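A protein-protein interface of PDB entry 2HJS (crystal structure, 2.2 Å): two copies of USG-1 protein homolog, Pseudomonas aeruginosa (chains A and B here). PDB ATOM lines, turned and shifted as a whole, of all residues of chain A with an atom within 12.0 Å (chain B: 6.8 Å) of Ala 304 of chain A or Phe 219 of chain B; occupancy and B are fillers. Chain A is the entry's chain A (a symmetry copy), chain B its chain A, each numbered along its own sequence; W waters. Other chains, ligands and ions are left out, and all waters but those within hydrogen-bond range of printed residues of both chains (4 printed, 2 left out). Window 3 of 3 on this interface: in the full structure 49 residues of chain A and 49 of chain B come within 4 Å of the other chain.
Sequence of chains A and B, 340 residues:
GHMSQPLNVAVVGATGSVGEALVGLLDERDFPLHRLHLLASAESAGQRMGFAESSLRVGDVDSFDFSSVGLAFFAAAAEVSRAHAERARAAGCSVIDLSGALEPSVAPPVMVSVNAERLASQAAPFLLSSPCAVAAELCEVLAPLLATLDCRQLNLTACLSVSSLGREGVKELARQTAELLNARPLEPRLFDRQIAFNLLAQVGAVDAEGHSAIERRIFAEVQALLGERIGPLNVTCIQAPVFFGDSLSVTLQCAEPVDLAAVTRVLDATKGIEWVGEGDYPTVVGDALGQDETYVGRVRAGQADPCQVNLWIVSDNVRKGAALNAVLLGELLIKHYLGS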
ATOM      1  N   THR A 251       1.147 -22.690 -21.915  1.00  0.00           N
ATOM      2  CA  THR A 251       0.025 -21.757 -22.123  1.00  0.00           C
ATOM      3  C   THR A 251      -1.269 -22.548 -22.187  1.00  0.00           C
ATOM      4  O   THR A 251      -1.405 -23.463 -23.005  1.00  0.00           O
ATOM      5  CB  THR A 251       0.143 -20.982 -23.434  1.00  0.00           C
ATOM      6  OG1 THR A 251       1.465 -20.475 -23.549  1.00  0.00           O
ATOM      7  CG2 THR A 251      -0.846 -19.797 -23.478  1.00  0.00           C
ATOM      8  N   LEU A 252      -2.208 -22.218 -21.314  1.00  0.00           N
ATOM      9  CA  LEU A 252      -3.525 -22.813 -21.371  1.00  0.00           C
ATOM     10  C   LEU A 252      -4.518 -21.806 -21.899  1.00  0.00           C
ATOM     11  O   LEU A 252      -4.571 -20.678 -21.410  1.00  0.00           O
ATOM     12  CB  LEU A 252      -4.002 -23.250 -19.979  1.00  0.00           C
ATOM     13  CG  LEU A 252      -3.050 -23.976 -19.028  1.00  0.00           C
ATOM     14  CD1 LEU A 252      -3.817 -24.485 -17.823  1.00  0.00           C
ATOM     15  CD2 LEU A 252      -2.494 -25.125 -19.779  1.00  0.00           C
ATOM     16  N   GLN A 253      -5.291 -22.217 -22.898  1.00  0.00           N
ATOM     17  CA  GLN A 253      -6.399 -21.427 -23.397  1.00  0.00           C
ATOM     18  C   GLN A 253      -7.666 -22.007 -22.799  1.00  0.00           C
ATOM     19  O   GLN A 253      -8.031 -23.153 -23.073  1.00  0.00           O
ATOM     20  CB  GLN A 253      -6.458 -21.490 -24.916  1.00  0.00           C
ATOM     21  CG  GLN A 253      -7.559 -20.640 -25.534  1.00  0.00           C
ATOM     22  CD  GLN A 253      -7.191 -19.178 -25.596  1.00  0.00           C
ATOM     23  OE1 GLN A 253      -6.102 -18.827 -26.033  1.00  0.00           O
ATOM     24  NE2 GLN A 253      -8.098 -18.314 -25.152  1.00  0.00           N
ATOM     25  N   CYS A 254      -8.327 -21.216 -21.965  1.00  0.00           N
ATOM     26  CA  CYS A 254      -9.490 -21.687 -21.250  1.00  0.00           C
ATOM     27  C   CYS A 254     -10.789 -21.130 -21.780  1.00  0.00           C
ATOM     28  O   CYS A 254     -10.791 -20.193 -22.561  1.00  0.00           O
ATOM     29  CB  CYS A 254      -9.344 -21.383 -19.767  1.00  0.00           C
ATOM     30  SG  CYS A 254      -7.819 -22.111 -19.123  1.00  0.00           S
ATOM     31  N   GLU A 256     -13.235 -19.728 -20.042  1.00  0.00           N
ATOM     32  CA  GLU A 256     -13.702 -18.603 -19.224  1.00  0.00           C
ATOM     33  C   GLU A 256     -12.465 -17.781 -18.808  1.00  0.00           C
ATOM     34  O   GLU A 256     -11.362 -18.337 -18.758  1.00  0.00           O
ATOM     35  CB  GLU A 256     -14.407 -19.142 -17.959  1.00  0.00           C
ATOM     36  CG  GLU A 256     -15.400 -20.316 -18.189  1.00  0.00           C
ATOM     37  CD  GLU A 256     -15.461 -21.310 -17.015  1.00  0.00           C
ATOM     38  OE1 GLU A 256     -15.043 -22.486 -17.198  1.00  0.00           O
ATOM     39  OE2 GLU A 256     -15.920 -20.917 -15.911  1.00  0.00           O
ATOM     40  N   PRO A 257     -12.628 -16.457 -18.539  1.00  0.00           N
ATOM     41  CA  PRO A 257     -11.505 -15.725 -17.911  1.00  0.00           C
ATOM     42  C   PRO A 257     -10.950 -16.447 -16.669  1.00  0.00           C
ATOM     43  O   PRO A 257     -11.716 -16.895 -15.808  1.00  0.00           O
ATOM     44  CB  PRO A 257     -12.132 -14.385 -17.524  1.00  0.00           C
ATOM     45  CG  PRO A 257     -13.230 -14.182 -18.554  1.00  0.00           C
ATOM     46  CD  PRO A 257     -13.778 -15.558 -18.815  1.00  0.00           C
ATOM     47  N   VAL A 258      -9.630 -16.586 -16.602  1.00  0.00           N
ATOM     48  CA  VAL A 258      -8.988 -17.355 -15.535  1.00  0.00           C
ATOM     49  C   VAL A 258      -8.885 -16.540 -14.251  1.00  0.00           C
ATOM     50  O   VAL A 258      -8.410 -15.404 -14.264  1.00  0.00           O
ATOM     51  CB  VAL A 258      -7.584 -17.860 -15.968  1.00  0.00           C
ATOM     52  CG1 VAL A 258      -6.925 -18.660 -14.864  1.00  0.00           C
ATOM     53  CG2 VAL A 258      -7.681 -18.726 -17.211  1.00  0.00           C
ATOM     54  N   LEU A 260      -6.814 -16.040 -11.607  1.00  0.00           N
ATOM     55  CA  LEU A 260      -5.399 -16.264 -11.318  1.00  0.00           C
ATOM     56  C   LEU A 260      -5.143 -16.593  -9.838  1.00  0.00           C
ATOM     57  O   LEU A 260      -4.409 -17.520  -9.528  1.00  0.00           O
ATOM     58  CB  LEU A 260      -4.570 -15.049 -11.770  1.00  0.00           C
ATOM     59  CG  LEU A 260      -4.601 -14.742 -13.274  1.00  0.00           C
ATOM     60  CD1 LEU A 260      -3.842 -13.448 -13.599  1.00  0.00           C
ATOM     61  CD2 LEU A 260      -4.102 -15.899 -14.116  1.00  0.00           C
ATOM     62  N   ARG A 298       5.388 -17.766 -12.467  1.00  0.00           N
ATOM     63  CA  ARG A 298       5.010 -16.872 -13.559  1.00  0.00           C
ATOM     64  C   ARG A 298       3.559 -17.060 -13.962  1.00  0.00           C
ATOM     65  O   ARG A 298       3.224 -16.955 -15.138  1.00  0.00           O
ATOM     66  CB  ARG A 298       5.957 -16.996 -14.779  1.00  0.00           C
ATOM     67  CG  ARG A 298       7.420 -16.645 -14.516  1.00  0.00           C
ATOM     68  CD  ARG A 298       8.055 -16.034 -15.748  1.00  0.00           C
ATOM     69  NE  ARG A 298       7.348 -14.819 -16.157  1.00  0.00           N
ATOM     70  CZ  ARG A 298       7.373 -14.272 -17.363  1.00  0.00           C
ATOM     71  NH1 ARG A 298       8.122 -14.805 -18.325  1.00  0.00           N
ATOM     72  NH2 ARG A 298       6.662 -13.159 -17.596  1.00  0.00           N
ATOM     73  N   ARG A 300       0.209 -16.024 -14.816  1.00  0.00           N
ATOM     74  CA  ARG A 300      -0.301 -14.735 -15.302  1.00  0.00           C
ATOM     75  C   ARG A 300      -1.290 -14.971 -16.444  1.00  0.00           C
ATOM     76  O   ARG A 300      -1.304 -16.054 -17.035  1.00  0.00           O
ATOM     77  CB  ARG A 300       0.861 -13.861 -15.808  1.00  0.00           C
ATOM     78  CG  ARG A 300       1.611 -14.503 -16.986  1.00  0.00           C
ATOM     79  CD  ARG A 300       2.964 -13.858 -17.213  1.00  0.00           C
ATOM     80  NE  ARG A 300       3.560 -14.217 -18.508  1.00  0.00           N
ATOM     81  CZ  ARG A 300       4.209 -15.363 -18.760  1.00  0.00           C
ATOM     82  NH1 ARG A 300       4.336 -16.308 -17.829  1.00  0.00           N
ATOM     83  NH2 ARG A 300       4.727 -15.578 -19.961  1.00  0.00           N
ATOM     84  N   ALA A 301      -2.095 -13.959 -16.752  1.00  0.00           N
ATOM     85  CA  ALA A 301      -2.959 -14.019 -17.908  1.00  0.00           C
ATOM     86  C   ALA A 301      -2.228 -13.500 -19.156  1.00  0.00           C
ATOM     87  O   ALA A 301      -1.132 -12.927 -19.053  1.00  0.00           O
ATOM     88  CB  ALA A 301      -4.215 -13.205 -17.668  1.00  0.00           C
ATOM     89  N   GLY A 302      -2.842 -13.712 -20.323  1.00  0.00           N
ATOM     90  CA  GLY A 302      -2.379 -13.118 -21.572  1.00  0.00           C
ATOM     91  C   GLY A 302      -2.444 -11.609 -21.439  1.00  0.00           C
ATOM     92  O   GLY A 302      -3.246 -11.074 -20.649  1.00  0.00           O
ATOM     93  N   GLN A 303      -1.607 -10.918 -22.207  1.00  0.00           N
ATOM     94  CA  GLN A 303      -1.602  -9.463 -22.205  1.00  0.00           C
ATOM     95  C   GLN A 303      -2.887  -8.988 -22.863  1.00  0.00           C
ATOM     96  O   GLN A 303      -3.452  -7.978 -22.464  1.00  0.00           O
ATOM     97  CB  GLN A 303      -0.355  -8.917 -22.925  1.00  0.00           C
ATOM     98  CG  GLN A 303       0.953  -9.275 -22.211  1.00  0.00           C
ATOM     99  CD  GLN A 303       2.204  -8.741 -22.915  1.00  0.00           C
ATOM    100  OE1 GLN A 303       2.343  -7.544 -23.107  1.00  0.00           O
ATOM    101  NE2 GLN A 303       3.113  -9.631 -23.283  1.00  0.00           N
ATOM    102  N   ALA A 304      -3.366  -9.763 -23.838  1.00  0.00           N
ATOM    103  CA  ALA A 304      -4.627  -9.464 -24.544  1.00  0.00           C
ATOM    104  C   ALA A 304      -5.852 -10.224 -23.958  1.00  0.00           C
ATOM    105  O   ALA A 304      -6.911  -9.620 -23.769  1.00  0.00           O
ATOM    106  CB  ALA A 304      -4.467  -9.783 -26.054  1.00  0.00           C
ATOM    107  N   ASP A 305      -5.661 -11.516 -23.645  1.00  0.00           N
ATOM    108  CA  ASP A 305      -6.731 -12.501 -23.401  1.00  0.00           C
ATOM    109  C   ASP A 305      -6.762 -12.953 -21.933  1.00  0.00           C
ATOM    110  O   ASP A 305      -5.873 -13.678 -21.498  1.00  0.00           O
ATOM    111  CB  ASP A 305      -6.459 -13.715 -24.313  1.00  0.00           C
ATOM    112  CG  ASP A 305      -7.680 -14.694 -24.482  1.00  0.00           C
ATOM    113  OD1 ASP A 305      -8.645 -14.777 -23.647  1.00  0.00           O
ATOM    114  OD2 ASP A 305      -7.616 -15.457 -25.494  1.00  0.00           O
ATOM    115  N   PRO A 306      -7.784 -12.517 -21.164  1.00  0.00           N
ATOM    116  CA  PRO A 306      -7.988 -13.041 -19.809  1.00  0.00           C
ATOM    117  C   PRO A 306      -8.297 -14.558 -19.772  1.00  0.00           C
ATOM    118  O   PRO A 306      -8.163 -15.168 -18.721  1.00  0.00           O
ATOM    119  CB  PRO A 306      -9.181 -12.229 -19.275  1.00  0.00           C
ATOM    120  CG  PRO A 306      -9.818 -11.613 -20.477  1.00  0.00           C
ATOM    121  CD  PRO A 306      -8.778 -11.484 -21.526  1.00  0.00           C
ATOM    122  N   CYS A 307      -8.691 -15.141 -20.907  1.00  0.00           N
ATOM    123  CA  CYS A 307      -8.965 -16.591 -20.996  1.00  0.00           C
ATOM    124  C   CYS A 307      -7.673 -17.445 -21.145  1.00  0.00           C
ATOM    125  O   CYS A 307      -7.745 -18.673 -21.215  1.00  0.00           O
ATOM    126  CB  CYS A 307      -9.936 -16.887 -22.154  1.00  0.00           C
ATOM    127  SG  CYS A 307     -11.549 -15.992 -22.103  1.00  0.00           S
ATOM    128  N   GLN A 308      -6.511 -16.785 -21.191  1.00  0.00           N
ATOM    129  CA  GLN A 308      -5.202 -17.444 -21.250  1.00  0.00           C
ATOM    130  C   GLN A 308      -4.475 -17.404 -19.917  1.00  0.00           C
ATOM    131  O   GLN A 308      -4.492 -16.384 -19.237  1.00  0.00           O
ATOM    132  CB  GLN A 308      -4.301 -16.730 -22.249  1.00  0.00           C
ATOM    133  CG  GLN A 308      -4.502 -17.135 -23.677  1.00  0.00           C
ATOM    134  CD  GLN A 308      -3.745 -16.254 -24.631  1.00  0.00           C
ATOM    135  OE1 GLN A 308      -2.822 -15.520 -24.248  1.00  0.00           O
ATOM    136  NE2 GLN A 308      -4.156 -16.283 -25.891  1.00  0.00           N
ATOM    137  N   VAL A 309      -3.819 -18.498 -19.550  1.00  0.00           N
ATOM    138  CA  VAL A 309      -2.973 -18.483 -18.362  1.00  0.00           C
ATOM    139  C   VAL A 309      -1.677 -19.166 -18.735  1.00  0.00           C
ATOM    140  O   VAL A 309      -1.693 -20.203 -19.397  1.00  0.00           O
ATOM    141  CB  VAL A 309      -3.660 -19.120 -17.080  1.00  0.00           C
ATOM    142  CG1 VAL A 309      -4.112 -20.570 -17.322  1.00  0.00           C
ATOM    143  CG2 VAL A 309      -2.730 -19.065 -15.837  1.00  0.00           C
ATOM    144  N   ASN A 310      -0.568 -18.557 -18.330  1.00  0.00           N
ATOM    145  CA  ASN A 310       0.762 -19.127 -18.510  1.00  0.00           C
ATOM    146  C   ASN A 310       1.260 -19.691 -17.212  1.00  0.00           C
ATOM    147  O   ASN A 310       0.918 -19.168 -16.165  1.00  0.00           O
ATOM    148  CB  ASN A 310       1.742 -18.044 -18.923  1.00  0.00           C
ATOM    149  CG  ASN A 310       1.489 -17.549 -20.313  1.00  0.00           C
ATOM    150  OD1 ASN A 310       0.738 -16.592 -20.517  1.00  0.00           O
ATOM    151  ND2 ASN A 310       2.062 -18.237 -21.295  1.00  0.00           N
ATOM    152  N   ALA B 135      10.674  -9.229 -31.959  1.00  0.00           N
ATOM    153  CA  ALA B 135       9.493  -8.834 -32.699  1.00  0.00           C
ATOM    154  C   ALA B 135       9.808  -8.736 -34.205  1.00  0.00           C
ATOM    155  O   ALA B 135       8.974  -9.108 -35.044  1.00  0.00           O
ATOM    156  CB  ALA B 135       8.975  -7.497 -32.201  1.00  0.00           C
ATOM    157  N   HIS B 211       4.159  -9.478 -16.484  1.00  0.00           N
ATOM    158  CA  HIS B 211       4.861  -9.415 -17.783  1.00  0.00           C
ATOM    159  C   HIS B 211       6.170  -8.653 -17.678  1.00  0.00           C
ATOM    160  O   HIS B 211       6.255  -7.656 -16.975  1.00  0.00           O
ATOM    161  CB  HIS B 211       3.946  -8.783 -18.862  1.00  0.00           C
ATOM    162  CG  HIS B 211       2.580  -9.395 -18.879  1.00  0.00           C
ATOM    163  ND1 HIS B 211       2.361 -10.692 -19.285  1.00  0.00           N
ATOM    164  CD2 HIS B 211       1.384  -8.925 -18.458  1.00  0.00           C
ATOM    165  CE1 HIS B 211       1.085 -10.995 -19.124  1.00  0.00           C
ATOM    166  NE2 HIS B 211       0.471  -9.945 -18.608  1.00  0.00           N
ATOM    167  N   ILE B 214      10.519  -6.707 -21.958  1.00  0.00           N
ATOM    168  CA  ILE B 214      10.717  -7.189 -23.331  1.00  0.00           C
ATOM    169  C   ILE B 214       9.434  -7.841 -23.884  1.00  0.00           C
ATOM    170  O   ILE B 214       9.115  -7.679 -25.044  1.00  0.00           O
ATOM    171  CB  ILE B 214      11.994  -8.102 -23.473  1.00  0.00           C
ATOM    172  CG1 ILE B 214      12.276  -8.417 -24.947  1.00  0.00           C
ATOM    173  CG2 ILE B 214      11.851  -9.413 -22.712  1.00  0.00           C
ATOM    174  CD1 ILE B 214      12.511  -7.196 -25.803  1.00  0.00           C
ATOM    175  N   GLU B 215       8.698  -8.539 -23.035  1.00  0.00           N
ATOM    176  CA  GLU B 215       7.422  -9.167 -23.406  1.00  0.00           C
ATOM    177  C   GLU B 215       6.343  -8.130 -23.801  1.00  0.00           C
ATOM    178  O   GLU B 215       5.607  -8.327 -24.781  1.00  0.00           O
ATOM    179  CB  GLU B 215       6.929 -10.035 -22.252  1.00  0.00           C
ATOM    180  CG  GLU B 215       7.637 -11.366 -22.188  1.00  0.00           C
ATOM    181  CD  GLU B 215       7.468 -12.103 -20.861  1.00  0.00           C
ATOM    182  OE1 GLU B 215       6.650 -11.676 -19.986  1.00  0.00           O
ATOM    183  OE2 GLU B 215       8.169 -13.132 -20.687  1.00  0.00           O
ATOM    184  N   ARG B 216       6.252  -7.059 -23.007  1.00  0.00           N
ATOM    185  CA  ARG B 216       5.418  -5.893 -23.295  1.00  0.00           C
ATOM    186  C   ARG B 216       5.797  -5.276 -24.625  1.00  0.00           C
ATOM    187  O   ARG B 216       4.928  -4.981 -25.457  1.00  0.00           O
ATOM    188  CB  ARG B 216       5.593  -4.848 -22.189  1.00  0.00           C
ATOM    189  CG  ARG B 216       4.408  -4.725 -21.251  1.00  0.00           C
ATOM    190  CD  ARG B 216       4.784  -4.524 -19.786  1.00  0.00           C
ATOM    191  NE  ARG B 216       5.789  -3.489 -19.492  1.00  0.00           N
ATOM    192  CZ  ARG B 216       6.698  -3.625 -18.525  1.00  0.00           C
ATOM    193  NH1 ARG B 216       6.735  -4.732 -17.784  1.00  0.00           N
ATOM    194  NH2 ARG B 216       7.569  -2.677 -18.294  1.00  0.00           N
ATOM    195  N   ARG B 217       7.097  -5.075 -24.823  1.00  0.00           N
ATOM    196  CA  ARG B 217       7.598  -4.460 -26.049  1.00  0.00           C
ATOM    197  C   ARG B 217       7.263  -5.298 -27.283  1.00  0.00           C
ATOM    198  O   ARG B 217       6.761  -4.780 -28.289  1.00  0.00           O
ATOM    199  CB  ARG B 217       9.095  -4.173 -25.972  1.00  0.00           C
ATOM    200  CG  ARG B 217       9.548  -3.322 -27.147  1.00  0.00           C
ATOM    201  CD  ARG B 217      11.045  -3.053 -27.179  1.00  0.00           C
ATOM    202  NE  ARG B 217      11.402  -2.390 -28.431  1.00  0.00           N
ATOM    203  CZ  ARG B 217      12.637  -2.015 -28.766  1.00  0.00           C
ATOM    204  NH1 ARG B 217      13.653  -2.241 -27.944  1.00  0.00           N
ATOM    205  NH2 ARG B 217      12.855  -1.434 -29.929  1.00  0.00           N
ATOM    206  N   ILE B 218       7.544  -6.596 -27.204  1.00  0.00           N
ATOM    207  CA  ILE B 218       7.298  -7.497 -28.315  1.00  0.00           C
ATOM    208  C   ILE B 218       5.806  -7.469 -28.642  1.00  0.00           C
ATOM    209  O   ILE B 218       5.410  -7.341 -29.814  1.00  0.00           O
ATOM    210  CB  ILE B 218       7.749  -8.944 -27.980  1.00  0.00           C
ATOM    211  CG1 ILE B 218       9.269  -9.048 -27.971  1.00  0.00           C
ATOM    212  CG2 ILE B 218       7.163  -9.929 -28.967  1.00  0.00           C
ATOM    213  CD1 ILE B 218       9.795 -10.222 -27.152  1.00  0.00           C
ATOM    214  N   PHE B 219       4.992  -7.565 -27.602  1.00  0.00           N
ATOM    215  CA  PHE B 219       3.558  -7.541 -27.760  1.00  0.00           C
ATOM    216  C   PHE B 219       3.084  -6.249 -28.447  1.00  0.00           C
ATOM    217  O   PHE B 219       2.341  -6.327 -29.412  1.00  0.00           O
ATOM    218  CB  PHE B 219       2.874  -7.711 -26.394  1.00  0.00           C
ATOM    219  CG  PHE B 219       1.361  -7.762 -26.457  1.00  0.00           C
ATOM    220  CD1 PHE B 219       0.699  -8.979 -26.621  1.00  0.00           C
ATOM    221  CD2 PHE B 219       0.613  -6.607 -26.349  1.00  0.00           C
ATOM    222  CE1 PHE B 219      -0.688  -9.046 -26.671  1.00  0.00           C
ATOM    223  CE2 PHE B 219      -0.788  -6.652 -26.405  1.00  0.00           C
ATOM    224  CZ  PHE B 219      -1.436  -7.879 -26.569  1.00  0.00           C
ATOM    225  N   ALA B 220       3.500  -5.082 -27.948  1.00  0.00           N
ATOM    226  CA  ALA B 220       3.077  -3.804 -28.524  1.00  0.00           C
ATOM    227  C   ALA B 220       3.507  -3.664 -29.979  1.00  0.00           C
ATOM    228  O   ALA B 220       2.755  -3.142 -30.811  1.00  0.00           O
ATOM    229  CB  ALA B 220       3.618  -2.620 -27.702  1.00  0.00           C
ATOM    230  N   GLU B 221       4.715  -4.131 -30.287  1.00  0.00           N
ATOM    231  CA  GLU B 221       5.273  -3.995 -31.647  1.00  0.00           C
ATOM    232  C   GLU B 221       4.608  -4.953 -32.626  1.00  0.00           C
ATOM    233  O   GLU B 221       4.280  -4.568 -33.741  1.00  0.00           O
ATOM    234  CB  GLU B 221       6.787  -4.188 -31.639  1.00  0.00           C
ATOM    235  CG  GLU B 221       7.491  -2.973 -31.053  1.00  0.00           C
ATOM    236  CD  GLU B 221       8.996  -3.159 -30.880  1.00  0.00           C
ATOM    237  OE1 GLU B 221       9.514  -4.307 -30.974  1.00  0.00           O
ATOM    238  OE2 GLU B 221       9.666  -2.147 -30.598  1.00  0.00           O
ATOM    239  N   VAL B 222       4.380  -6.195 -32.203  1.00  0.00           N
ATOM    240  CA  VAL B 222       3.700  -7.143 -33.083  1.00  0.00           C
ATOM    241  C   VAL B 222       2.294  -6.639 -33.430  1.00  0.00           C
ATOM    242  O   VAL B 222       1.854  -6.728 -34.581  1.00  0.00           O
ATOM    243  CB  VAL B 222       3.715  -8.558 -32.494  1.00  0.00           C
ATOM    244  CG1 VAL B 222       2.891  -9.537 -33.329  1.00  0.00           C
ATOM    245  CG2 VAL B 222       5.145  -9.042 -32.419  1.00  0.00           C
ATOM    246  N   GLN B 223       1.600  -6.062 -32.455  1.00  0.00           N
ATOM    247  CA  GLN B 223       0.258  -5.545 -32.715  1.00  0.00           C
ATOM    248  C   GLN B 223       0.269  -4.260 -33.552  1.00  0.00           C
ATOM    249  O   GLN B 223      -0.669  -4.013 -34.305  1.00  0.00           O
ATOM    250  CB  GLN B 223      -0.570  -5.425 -31.422  1.00  0.00           C
ATOM    251  CG  GLN B 223      -0.910  -4.025 -30.861  1.00  0.00           C
ATOM    252  CD  GLN B 223      -1.843  -4.133 -29.631  1.00  0.00           C
ATOM    253  OE1 GLN B 223      -2.412  -5.191 -29.361  1.00  0.00           O
ATOM    254  NE2 GLN B 223      -1.986  -3.045 -28.893  1.00  0.00           N
ATOM    255  N   ALA B 224       1.328  -3.458 -33.436  1.00  0.00           N
ATOM    256  CA  ALA B 224       1.473  -2.280 -34.310  1.00  0.00           C
ATOM    257  C   ALA B 224       1.849  -2.699 -35.720  1.00  0.00           C
ATOM    258  O   ALA B 224       1.322  -2.157 -36.665  1.00  0.00           O
ATOM    259  CB  ALA B 224       2.454  -1.263 -33.766  1.00  0.00           C
ATOM    260  N   GLY B 231      -4.700 -12.983 -34.400  1.00  0.00           N
ATOM    261  CA  GLY B 231      -5.443 -12.946 -33.152  1.00  0.00           C
ATOM    262  C   GLY B 231      -4.518 -12.729 -31.965  1.00  0.00           C
ATOM    263  O   GLY B 231      -3.349 -12.383 -32.133  1.00  0.00           O
ATOM    264  N   PRO B 232      -5.021 -12.986 -30.754  1.00  0.00           N
ATOM    265  CA  PRO B 232      -4.233 -12.735 -29.547  1.00  0.00           C
ATOM    266  C   PRO B 232      -2.805 -13.332 -29.639  1.00  0.00           C
ATOM    267  O   PRO B 232      -2.638 -14.492 -30.049  1.00  0.00           O
ATOM    268  CB  PRO B 232      -5.024 -13.463 -28.464  1.00  0.00           C
ATOM    269  CG  PRO B 232      -6.418 -13.557 -28.999  1.00  0.00           C
ATOM    270  CD  PRO B 232      -6.336 -13.582 -30.469  1.00  0.00           C
ATOM    271  N   LEU B 233      -1.802 -12.520 -29.306  1.00  0.00           N
ATOM    272  CA  LEU B 233      -0.432 -12.971 -29.128  1.00  0.00           C
ATOM    273  C   LEU B 233      -0.164 -13.368 -27.663  1.00  0.00           C
ATOM    274  O   LEU B 233      -0.497 -12.624 -26.755  1.00  0.00           O
ATOM    275  CB  LEU B 233       0.497 -11.829 -29.440  1.00  0.00           C
ATOM    276  CG  LEU B 233       1.926 -12.065 -29.920  1.00  0.00           C
ATOM    277  CD1 LEU B 233       2.872 -10.977 -29.350  1.00  0.00           C
ATOM    278  CD2 LEU B 233       2.492 -13.440 -29.689  1.00  0.00           C
ATOM    279  N   ASN B 234       0.480 -14.507 -27.443  1.00  0.00           N
ATOM    280  CA  ASN B 234       0.961 -14.850 -26.110  1.00  0.00           C
ATOM    281  C   ASN B 234       2.482 -15.029 -26.155  1.00  0.00           C
ATOM    282  O   ASN B 234       2.981 -15.817 -26.959  1.00  0.00           O
ATOM    283  CB  ASN B 234       0.225 -16.096 -25.593  1.00  0.00           C
ATOM    284  CG  ASN B 234       0.610 -16.466 -24.178  1.00  0.00           C
ATOM    285  OD1 ASN B 234       1.692 -17.011 -23.940  1.00  0.00           O
ATOM    286  ND2 ASN B 234      -0.305 -16.231 -23.230  1.00  0.00           N
ATOM    287  N   VAL B 235       3.205 -14.251 -25.330  1.00  0.00           N
ATOM    288  CA  VAL B 235       4.677 -14.159 -25.390  1.00  0.00           C
ATOM    289  C   VAL B 235       5.310 -14.527 -24.070  1.00  0.00           C
ATOM    290  O   VAL B 235       4.976 -13.927 -23.064  1.00  0.00           O
ATOM    291  CB  VAL B 235       5.211 -12.716 -25.553  1.00  0.00           C
ATOM    292  CG1 VAL B 235       6.659 -12.740 -26.086  1.00  0.00           C
ATOM    293  CG2 VAL B 235       4.349 -11.895 -26.391  1.00  0.00           C
HETATM  294  O   HOH W   1      -2.617 -16.515 -28.256  1.00  0.00           O
HETATM  295  O   HOH W   2      -2.269  -9.664 -18.313  1.00  0.00           O
HETATM  296  O   HOH W   3      -2.543 -12.742 -24.936  1.00  0.00           O
HETATM  297  O   HOH W   4       4.036 -12.025 -20.836  1.00  0.00           O
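NE2 of His 211 of chain B lies close to O of Ala 301 of chain A, 3.4 Å away. The side-chain carboxylate of Glu 215 of chain B lies within salt-bridge range of the guanidinium group of Arg 298 of chain A (2.8 Å). The backbone carbonyl oxygen (O) of Glu 215 of chain B lies within hydrogen-bond range of the side-chain amide nitrogen (NE2) of Gln 303 of chain A (3.2 Å). The side-chain hydroxyl (OG1) of Thr 251 of chain A sits at hydrogen-bond distance from the side-chain amide oxygen (OD1) of Asn 234 of chain B, 3.5 Å away. The side-chain amide oxygen (OE1) of Gln 308 of chain A lies within hydrogen-bond range of the side-chain amide nitrogen (ND2) of Asn 234 of chain B (2.8 Å). The side-chain amide oxygen (OD1) of Asn 310 of chain A is in hydrogen-bond range of the side-chain amide nitrogen (ND2) of Asn 234 of chain B (2.9 Å).
The backbone carbonyl oxygen (O) of His 211 of chain B sits at hydrogen-bond distance from the guanidinium group (NH1) of Arg 216 of chain B, at 3.1 Å. The side-chain amide nitrogen (NE2) of Gln 308 of chain A is in hydrogen-bond range of the side-chain amide oxygen (OE1) of Gln 253 of chain A (3.2 Å).
Among the printed residues, merely in contact across the chains: Gln 303 of chain A with Phe 219 of chain B (3.3 Å), Gln 303 of chain A with Arg 216 of chain B (3.5 Å), Arg 300 of chain A with Val 235 of chain B (3.5 Å), Gln 303 of chain A with His 211 of chain B (3.5 Å), Ala 304 of chain A with Phe 219 of chain B (3.6 Å), Arg 300 of chain A with His 211 of chain B (3.8 Å) and Gln 308 of chain A with Pro 232 of chain B (3.9 Å).
Printed residues of chain B within 4 Å of Thr 251 of chain A: Asn 234. Of chain B, only Phe 219 (3.6 Å) comes within 4 Å of Ala 304 of chain A. Of the printed residues of chain B, Gln 308 of chain A touches Pro 232 (3.9 Å) and Asn 234 (2.8 Å). No residue of chain A comes within 4 Å of Ile 218 of chain B. Of the printed residues of chain A, Phe 219 of chain B touches Gln 303 and Ala 304. No residue of chain A comes within 4 Å of Ala 220 of chain B. No residue of chain A comes within 4 Å of Val 222 of chain B. Pro 232 of chain B touches just one residue of chain A: Gln 308 (3.9 Å). Printed residues of chain A within 4 Å of Asn 234 of chain B: Thr 251 (3.5 Å), Gln 308 (2.8 Å) and Asn 310 (2.9 Å).
Of the 20 printed residues of chain A, 8 touch a printed residue of chain B. Hydrophobic or aromatic side chains of chain A that line the printed part of chain B: Ala 304. Of the 18 printed residues of chain B, 7 touch a printed residue of chain A. Printed residues of chain B that touch a printed residue of chain A: His 211, Glu 215, Arg 216, Phe 219, Pro 232, Asn 234 and Val 235. Hydrophobic or aromatic side chains of chain B that line the printed part of chain A: His 211, Phe 219 and Pro 232.
No position is printed for both chains. Of the 13 pairs that touch across the chains among the printed residues, none has its exchanged pair printed and touching as well.
Water W1 bridges O of Pro 232 of chain B (2.7 Å) and NE2 of Gln 308 of chain A (2.8 Å). Water W3 lies within hydrogen-bond range of O of Leu 233 of chain B (2.7 Å), OE1 of Gln 308 of chain A (2.9 Å), N of Ala 304 of chain A (3.3 Å) and N of Gln 303 of chain A (3.4 Å).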
